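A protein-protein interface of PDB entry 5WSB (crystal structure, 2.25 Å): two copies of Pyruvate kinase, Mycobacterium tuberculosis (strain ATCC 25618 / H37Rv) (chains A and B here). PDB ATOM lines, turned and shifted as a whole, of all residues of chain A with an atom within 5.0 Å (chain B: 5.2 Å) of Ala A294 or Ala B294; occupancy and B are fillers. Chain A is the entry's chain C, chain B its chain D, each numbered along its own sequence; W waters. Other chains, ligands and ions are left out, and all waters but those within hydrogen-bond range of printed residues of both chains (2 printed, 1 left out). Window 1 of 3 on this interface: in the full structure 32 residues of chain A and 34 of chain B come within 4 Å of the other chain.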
ATOM      1  N   ARG A 245       8.724   2.757   7.160  1.00  0.00           N
ATOM      2  CA  ARG A 245       7.510   2.599   7.961  1.00  0.00           C
ATOM      3  C   ARG A 245       7.208   1.165   8.304  1.00  0.00           C
ATOM      4  O   ARG A 245       6.529   0.904   9.288  1.00  0.00           O
ATOM      5  CB  ARG A 245       6.332   3.240   7.229  1.00  0.00           C
ATOM      6  CG  ARG A 245       6.554   4.717   6.970  1.00  0.00           C
ATOM      7  CD  ARG A 245       5.345   5.434   6.412  1.00  0.00           C
ATOM      8  NE  ARG A 245       4.744   4.729   5.300  1.00  0.00           N
ATOM      9  CZ  ARG A 245       3.627   5.126   4.692  1.00  0.00           C
ATOM     10  NH1 ARG A 245       3.131   4.415   3.694  1.00  0.00           N
ATOM     11  NH2 ARG A 245       3.001   6.246   5.087  1.00  0.00           N
ATOM     12  N   GLN A 280       4.547   0.222   1.888  1.00  0.00           N
ATOM     13  CA  GLN A 280       3.109  -0.017   1.861  1.00  0.00           C
ATOM     14  C   GLN A 280       2.268   1.141   1.337  1.00  0.00           C
ATOM     15  O   GLN A 280       1.050   1.147   1.532  1.00  0.00           O
ATOM     16  CB  GLN A 280       2.585  -0.489   3.241  1.00  0.00           C
ATOM     17  CG  GLN A 280       3.121  -1.867   3.656  1.00  0.00           C
ATOM     18  CD  GLN A 280       2.308  -2.527   4.783  1.00  0.00           C
ATOM     19  OE1 GLN A 280       1.944  -1.886   5.782  1.00  0.00           O
ATOM     20  NE2 GLN A 280       2.051  -3.817   4.640  1.00  0.00           N
ATOM     21  N   MET A 281       2.889   2.113   0.681  1.00  0.00           N
ATOM     22  CA  MET A 281       2.142   3.252   0.151  1.00  0.00           C
ATOM     23  C   MET A 281       1.063   2.790  -0.815  1.00  0.00           C
ATOM     24  O   MET A 281      -0.043   3.336  -0.833  1.00  0.00           O
ATOM     25  CB  MET A 281       3.070   4.245  -0.563  1.00  0.00           C
ATOM     26  CG  MET A 281       4.113   4.848   0.357  1.00  0.00           C
ATOM     27  SD  MET A 281       4.659   6.529  -0.058  1.00  0.00           S
ATOM     28  CE  MET A 281       3.403   7.495   0.770  1.00  0.00           C
ATOM     29  N   THR A 292      -6.137   0.915  -2.880  1.00  0.00           N
ATOM     30  CA  THR A 292      -7.277   1.260  -2.011  1.00  0.00           C
ATOM     31  C   THR A 292      -7.378   2.781  -1.908  1.00  0.00           C
ATOM     32  O   THR A 292      -6.517   3.522  -2.413  1.00  0.00           O
ATOM     33  CB  THR A 292      -7.122   0.636  -0.617  1.00  0.00           C
ATOM     34  OG1 THR A 292      -5.969   1.188   0.030  1.00  0.00           O
ATOM     35  CG2 THR A 292      -6.968  -0.888  -0.749  1.00  0.00           C
ATOM     36  N   ARG A 293      -8.438   3.242  -1.270  1.00  0.00           N
ATOM     37  CA  ARG A 293      -8.666   4.666  -1.088  1.00  0.00           C
ATOM     38  C   ARG A 293      -7.734   5.144   0.006  1.00  0.00           C
ATOM     39  O   ARG A 293      -7.253   6.267  -0.030  1.00  0.00           O
ATOM     40  CB  ARG A 293     -10.125   4.928  -0.705  1.00  0.00           C
ATOM     41  CG  ARG A 293     -11.158   4.329  -1.628  1.00  0.00           C
ATOM     42  CD  ARG A 293     -11.038   4.899  -3.042  1.00  0.00           C
ATOM     43  NE  ARG A 293     -11.965   4.310  -3.990  1.00  0.00           N
ATOM     44  CZ  ARG A 293     -11.803   3.126  -4.584  1.00  0.00           C
ATOM     45  NH1 ARG A 293     -10.772   2.352  -4.283  1.00  0.00           N
ATOM     46  NH2 ARG A 293     -12.689   2.705  -5.469  1.00  0.00           N
ATOM     47  N   ALA A 294      -7.455   4.275   0.974  1.00  0.00           N
ATOM     48  CA  ALA A 294      -6.432   4.592   1.985  1.00  0.00           C
ATOM     49  C   ALA A 294      -5.079   4.812   1.342  1.00  0.00           C
ATOM     50  O   ALA A 294      -4.328   5.700   1.719  1.00  0.00           O
ATOM     51  CB  ALA A 294      -6.339   3.478   3.018  1.00  0.00           C
ATOM     52  N   GLU A 295      -4.745   3.963   0.393  1.00  0.00           N
ATOM     53  CA  GLU A 295      -3.441   4.024  -0.256  1.00  0.00           C
ATOM     54  C   GLU A 295      -3.283   5.286  -1.079  1.00  0.00           C
ATOM     55  O   GLU A 295      -2.239   5.956  -1.022  1.00  0.00           O
ATOM     56  CB  GLU A 295      -3.254   2.777  -1.094  1.00  0.00           C
ATOM     57  CG  GLU A 295      -2.792   1.605  -0.262  1.00  0.00           C
ATOM     58  CD  GLU A 295      -3.055   0.245  -0.881  1.00  0.00           C
ATOM     59  OE1 GLU A 295      -3.609   0.156  -2.033  1.00  0.00           O
ATOM     60  OE2 GLU A 295      -2.703  -0.752  -0.193  1.00  0.00           O
ATOM     61  N   ALA A 296      -4.301   5.626  -1.849  1.00  0.00           N
ATOM     62  CA  ALA A 296      -4.256   6.840  -2.647  1.00  0.00           C
ATOM     63  C   ALA A 296      -4.169   8.078  -1.732  1.00  0.00           C
ATOM     64  O   ALA A 296      -3.474   9.059  -2.031  1.00  0.00           O
ATOM     65  CB  ALA A 296      -5.470   6.918  -3.542  1.00  0.00           C
ATOM     66  N   SER A 297      -4.872   8.030  -0.621  1.00  0.00           N
ATOM     67  CA  SER A 297      -4.769   9.075   0.402  1.00  0.00           C
ATOM     68  C   SER A 297      -3.337   9.167   0.966  1.00  0.00           C
ATOM     69  O   SER A 297      -2.803  10.258   1.195  1.00  0.00           O
ATOM     70  CB  SER A 297      -5.784   8.766   1.552  1.00  0.00           C
ATOM     71  OG  SER A 297      -5.659   9.667   2.657  1.00  0.00           O
ATOM     72  N   ASP A 298      -2.740   8.022   1.248  1.00  0.00           N
ATOM     73  CA  ASP A 298      -1.461   8.001   1.952  1.00  0.00           C
ATOM     74  C   ASP A 298      -0.388   8.660   1.068  1.00  0.00           C
ATOM     75  O   ASP A 298       0.448   9.426   1.552  1.00  0.00           O
ATOM     76  CB  ASP A 298      -1.087   6.558   2.285  1.00  0.00           C
ATOM     77  CG  ASP A 298       0.276   6.440   2.919  1.00  0.00           C
ATOM     78  OD1 ASP A 298       0.602   7.264   3.797  1.00  0.00           O
ATOM     79  OD2 ASP A 298       1.013   5.482   2.584  1.00  0.00           O
ATOM     80  N   ARG B 245     -16.157   7.109  -0.528  1.00  0.00           N
ATOM     81  CA  ARG B 245     -14.967   7.103  -1.366  1.00  0.00           C
ATOM     82  C   ARG B 245     -14.929   5.924  -2.318  1.00  0.00           C
ATOM     83  O   ARG B 245     -14.282   5.988  -3.358  1.00  0.00           O
ATOM     84  CB  ARG B 245     -13.724   7.131  -0.473  1.00  0.00           C
ATOM     85  CG  ARG B 245     -13.688   8.371   0.420  1.00  0.00           C
ATOM     86  CD  ARG B 245     -12.409   8.536   1.206  1.00  0.00           C
ATOM     87  NE  ARG B 245     -11.991   7.312   1.876  1.00  0.00           N
ATOM     88  CZ  ARG B 245     -10.830   7.190   2.521  1.00  0.00           C
ATOM     89  NH1 ARG B 245     -10.508   6.032   3.060  1.00  0.00           N
ATOM     90  NH2 ARG B 245      -9.982   8.237   2.618  1.00  0.00           N
ATOM     91  N   GLN B 280     -12.865   1.865   3.005  1.00  0.00           N
ATOM     92  CA  GLN B 280     -11.510   1.345   2.888  1.00  0.00           C
ATOM     93  C   GLN B 280     -10.455   2.002   3.771  1.00  0.00           C
ATOM     94  O   GLN B 280      -9.258   1.855   3.523  1.00  0.00           O
ATOM     95  CB  GLN B 280     -11.071   1.323   1.417  1.00  0.00           C
ATOM     96  CG  GLN B 280     -11.912   0.360   0.575  1.00  0.00           C
ATOM     97  CD  GLN B 280     -11.475   0.255  -0.863  1.00  0.00           C
ATOM     98  OE1 GLN B 280     -10.890   1.169  -1.444  1.00  0.00           O
ATOM     99  NE2 GLN B 280     -11.740  -0.896  -1.444  1.00  0.00           N
ATOM    100  N   MET B 281     -10.877   2.717   4.798  1.00  0.00           N
ATOM    101  CA  MET B 281      -9.933   3.347   5.727  1.00  0.00           C
ATOM    102  C   MET B 281      -8.996   2.315   6.336  1.00  0.00           C
ATOM    103  O   MET B 281      -7.805   2.564   6.522  1.00  0.00           O
ATOM    104  CB  MET B 281     -10.684   4.093   6.849  1.00  0.00           C
ATOM    105  CG  MET B 281     -11.564   5.214   6.319  1.00  0.00           C
ATOM    106  SD  MET B 281     -11.755   6.683   7.382  1.00  0.00           S
ATOM    107  CE  MET B 281     -10.277   7.593   6.981  1.00  0.00           C
ATOM    108  N   THR B 292      -2.402  -1.746   7.190  1.00  0.00           N
ATOM    109  CA  THR B 292      -1.180  -1.308   6.489  1.00  0.00           C
ATOM    110  C   THR B 292      -0.766   0.075   7.018  1.00  0.00           C
ATOM    111  O   THR B 292      -1.476   0.701   7.820  1.00  0.00           O
ATOM    112  CB  THR B 292      -1.409  -1.234   4.972  1.00  0.00           C
ATOM    113  OG1 THR B 292      -2.404  -0.252   4.688  1.00  0.00           O
ATOM    114  CG2 THR B 292      -1.870  -2.576   4.441  1.00  0.00           C
ATOM    115  N   ARG B 293       0.396   0.545   6.580  1.00  0.00           N
ATOM    116  CA  ARG B 293       0.890   1.844   7.006  1.00  0.00           C
ATOM    117  C   ARG B 293       0.128   2.909   6.224  1.00  0.00           C
ATOM    118  O   ARG B 293      -0.117   4.003   6.730  1.00  0.00           O
ATOM    119  CB  ARG B 293       2.374   1.954   6.771  1.00  0.00           C
ATOM    120  CG  ARG B 293       3.204   0.866   7.407  1.00  0.00           C
ATOM    121  CD  ARG B 293       3.157   0.887   8.921  1.00  0.00           C
ATOM    122  NE  ARG B 293       3.799  -0.315   9.409  1.00  0.00           N
ATOM    123  CZ  ARG B 293       3.167  -1.351   9.967  1.00  0.00           C
ATOM    124  NH1 ARG B 293       1.849  -1.319  10.192  1.00  0.00           N
ATOM    125  NH2 ARG B 293       3.857  -2.405  10.362  1.00  0.00           N
ATOM    126  N   ALA B 294      -0.276   2.580   4.995  1.00  0.00           N
ATOM    127  CA  ALA B 294      -1.201   3.464   4.254  1.00  0.00           C
ATOM    128  C   ALA B 294      -2.497   3.698   5.033  1.00  0.00           C
ATOM    129  O   ALA B 294      -3.037   4.795   5.098  1.00  0.00           O
ATOM    130  CB  ALA B 294      -1.530   2.861   2.898  1.00  0.00           C
ATOM    131  N   GLU B 295      -3.029   2.623   5.573  1.00  0.00           N
ATOM    132  CA  GLU B 295      -4.320   2.678   6.244  1.00  0.00           C
ATOM    133  C   GLU B 295      -4.250   3.479   7.519  1.00  0.00           C
ATOM    134  O   GLU B 295      -5.128   4.321   7.787  1.00  0.00           O
ATOM    135  CB  GLU B 295      -4.786   1.265   6.494  1.00  0.00           C
ATOM    136  CG  GLU B 295      -5.425   0.666   5.264  1.00  0.00           C
ATOM    137  CD  GLU B 295      -5.467  -0.829   5.253  1.00  0.00           C
ATOM    138  OE1 GLU B 295      -5.002  -1.499   6.246  1.00  0.00           O
ATOM    139  OE2 GLU B 295      -5.968  -1.341   4.216  1.00  0.00           O
ATOM    140  N   ALA B 296      -3.212   3.246   8.309  1.00  0.00           N
ATOM    141  CA  ALA B 296      -3.019   3.998   9.529  1.00  0.00           C
ATOM    142  C   ALA B 296      -2.843   5.497   9.220  1.00  0.00           C
ATOM    143  O   ALA B 296      -3.372   6.371   9.938  1.00  0.00           O
ATOM    144  CB  ALA B 296      -1.814   3.463  10.287  1.00  0.00           C
ATOM    145  N   SER B 297      -2.096   5.786   8.171  1.00  0.00           N
ATOM    146  CA  SER B 297      -1.972   7.158   7.678  1.00  0.00           C
ATOM    147  C   SER B 297      -3.338   7.760   7.272  1.00  0.00           C
ATOM    148  O   SER B 297      -3.624   8.946   7.517  1.00  0.00           O
ATOM    149  CB  SER B 297      -1.005   7.172   6.444  1.00  0.00           C
ATOM    150  OG  SER B 297      -0.886   8.473   5.850  1.00  0.00           O
ATOM    151  N   ASP B 298      -4.137   6.979   6.567  1.00  0.00           N
ATOM    152  CA  ASP B 298      -5.357   7.518   5.952  1.00  0.00           C
ATOM    153  C   ASP B 298      -6.316   7.957   7.061  1.00  0.00           C
ATOM    154  O   ASP B 298      -6.958   9.022   6.976  1.00  0.00           O
ATOM    155  CB  ASP B 298      -6.003   6.453   5.065  1.00  0.00           C
ATOM    156  CG  ASP B 298      -7.328   6.905   4.481  1.00  0.00           C
ATOM    157  OD1 ASP B 298      -7.420   8.066   4.036  1.00  0.00           O
ATOM    158  OD2 ASP B 298      -8.282   6.090   4.437  1.00  0.00           O
ATOM    159  N   VAL B 299      -6.354   7.155   8.124  1.00  0.00           N
ATOM    160  CA  VAL B 299      -7.124   7.469   9.332  1.00  0.00           C
ATOM    161  C   VAL B 299      -6.629   8.714  10.055  1.00  0.00           C
ATOM    162  O   VAL B 299      -7.424   9.593  10.391  1.00  0.00           O
ATOM    163  CB  VAL B 299      -7.104   6.286  10.319  1.00  0.00           C
ATOM    164  CG1 VAL B 299      -7.620   6.728  11.689  1.00  0.00           C
ATOM    165  CG2 VAL B 299      -7.930   5.121   9.783  1.00  0.00           C
HETATM  166  O   HOH W   1      -7.035   0.272   2.588  1.00  0.00           O
HETATM  167  O   HOH W   2      -7.870  10.786   4.459  1.00  0.00           O
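Of chain B, only Gln B280, Met B281, Ala B294, Glu B295 and Asp B298 come within 4 Å of Ala A294.
Printed residues of chain A within 4 Å of Gln B280: Thr A292 (3.7 Å), Arg A293 (3.1 Å) and Ala A294 (3.4 Å).
Printed residues of chain A within 4 Å of Ser B297: Asp A298.
The nearest residue of chain B that does not touch Ala A294 is Arg B245 (4.1 Å).
The nearest residue of chain A that does not touch Ala B294 is Met A281 (4.04 Å).
The nearest printed residue of chain A that does not touch Glu B295 is Thr A292 (4.9 Å).
N of Thr B292 lies within hydrogen-bond range of OE1 of Glu B295 (2.8 Å).
The side-chain carboxylate (OD2) of Asp B298 lies within salt-bridge range of the guanidinium group (NH1) of Arg B245.
OD2 of Asp A298 lies within salt-bridge range of NH1 of Arg A245 (2.6 Å).
The backbone NH of Thr A292 sits at hydrogen-bond distance from the side-chain carboxylate of Glu A295.
Printed residues of chain A that touch a printed residue of chain B: Arg A245, Gln A280, Thr A292, Arg A293, Ala A294, Glu A295, Ser A297 and Asp A298.
Hydrophobic or aromatic side chains of chain A within 4 Å of the printed part of chain B: Ala A294.
Along chain B the printed residues that touch a printed residue of chain A span positions 245 to 298.
Among the printed residues, no Asp or Glu carboxylate lies within 4 Å of a Lys or Arg side-chain nitrogen of the other chain.
Arg A245 touches Arg B293, and with the chains exchanged Arg A293 touches Arg B245.
Gln A280 touches Thr B292, and with the chains exchanged Thr A292 touches Gln B280.
Gln A280 touches Arg B293, and with the chains exchanged Arg A293 touches Gln B280.
Ala A294 touches Asp B298, and with the chains exchanged Asp A298 touches Ala B294.
10 positions are printed for both chains.
Of the 16 pairs that touch across the chains among the printed residues, 15 have their exchanged pair printed and touching as well.
Among the printed residues, pairs that only touch across the chains: Gln A280 with Thr B292, Gln A280 with Ala B294, Thr A292 with Gln B280, Ala A294 with Gln B280, Ala A294 with Met B281, Ala A294 with Ala B294, Ala A294 with Glu B295, Ala A294 with Asp B298, Glu A295 with Ala B294 and Asp A298 with Ala B294.
The side-chain carboxylate (OD1) of Asp A298 lies within hydrogen-bond range of the side-chain hydroxyl (OG) of Ser B297.
NE of Arg A293 is in hydrogen-bond range of O of Arg B245 (2.9 Å).
The side-chain amide oxygen of Gln A280 is in hydrogen-bond range of the backbone NH of Arg B293, 3.0 Å away.
The side-chain hydroxyl (OG) of Ser A297 is in hydrogen-bond range of the side-chain carboxylate (OD1) of Asp B298, 2.8 Å away.
The guanidinium group (NE) of Arg B293 sits at hydrogen-bond distance from the backbone carbonyl oxygen (O) of Arg A245 (3.0 Å).
The guanidinium group (NH1) of Arg A293 sits at hydrogen-bond distance from the side-chain amide oxygen (OE1) of Gln B280 (3.1 Å).
Water W1 lies within hydrogen-bond range of the side-chain carboxylate (OE2) of Glu B295, the backbone carbonyl oxygen (O) of Gln B280 and the side-chain hydroxyl (OG1) of Thr A292.
Water W2 lies within hydrogen-bond range of the side-chain carboxylate (OD1) of Asp B298 (2.8 Å) and the side-chain hydroxyl (OG) of Ser A297 (3.1 Å).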
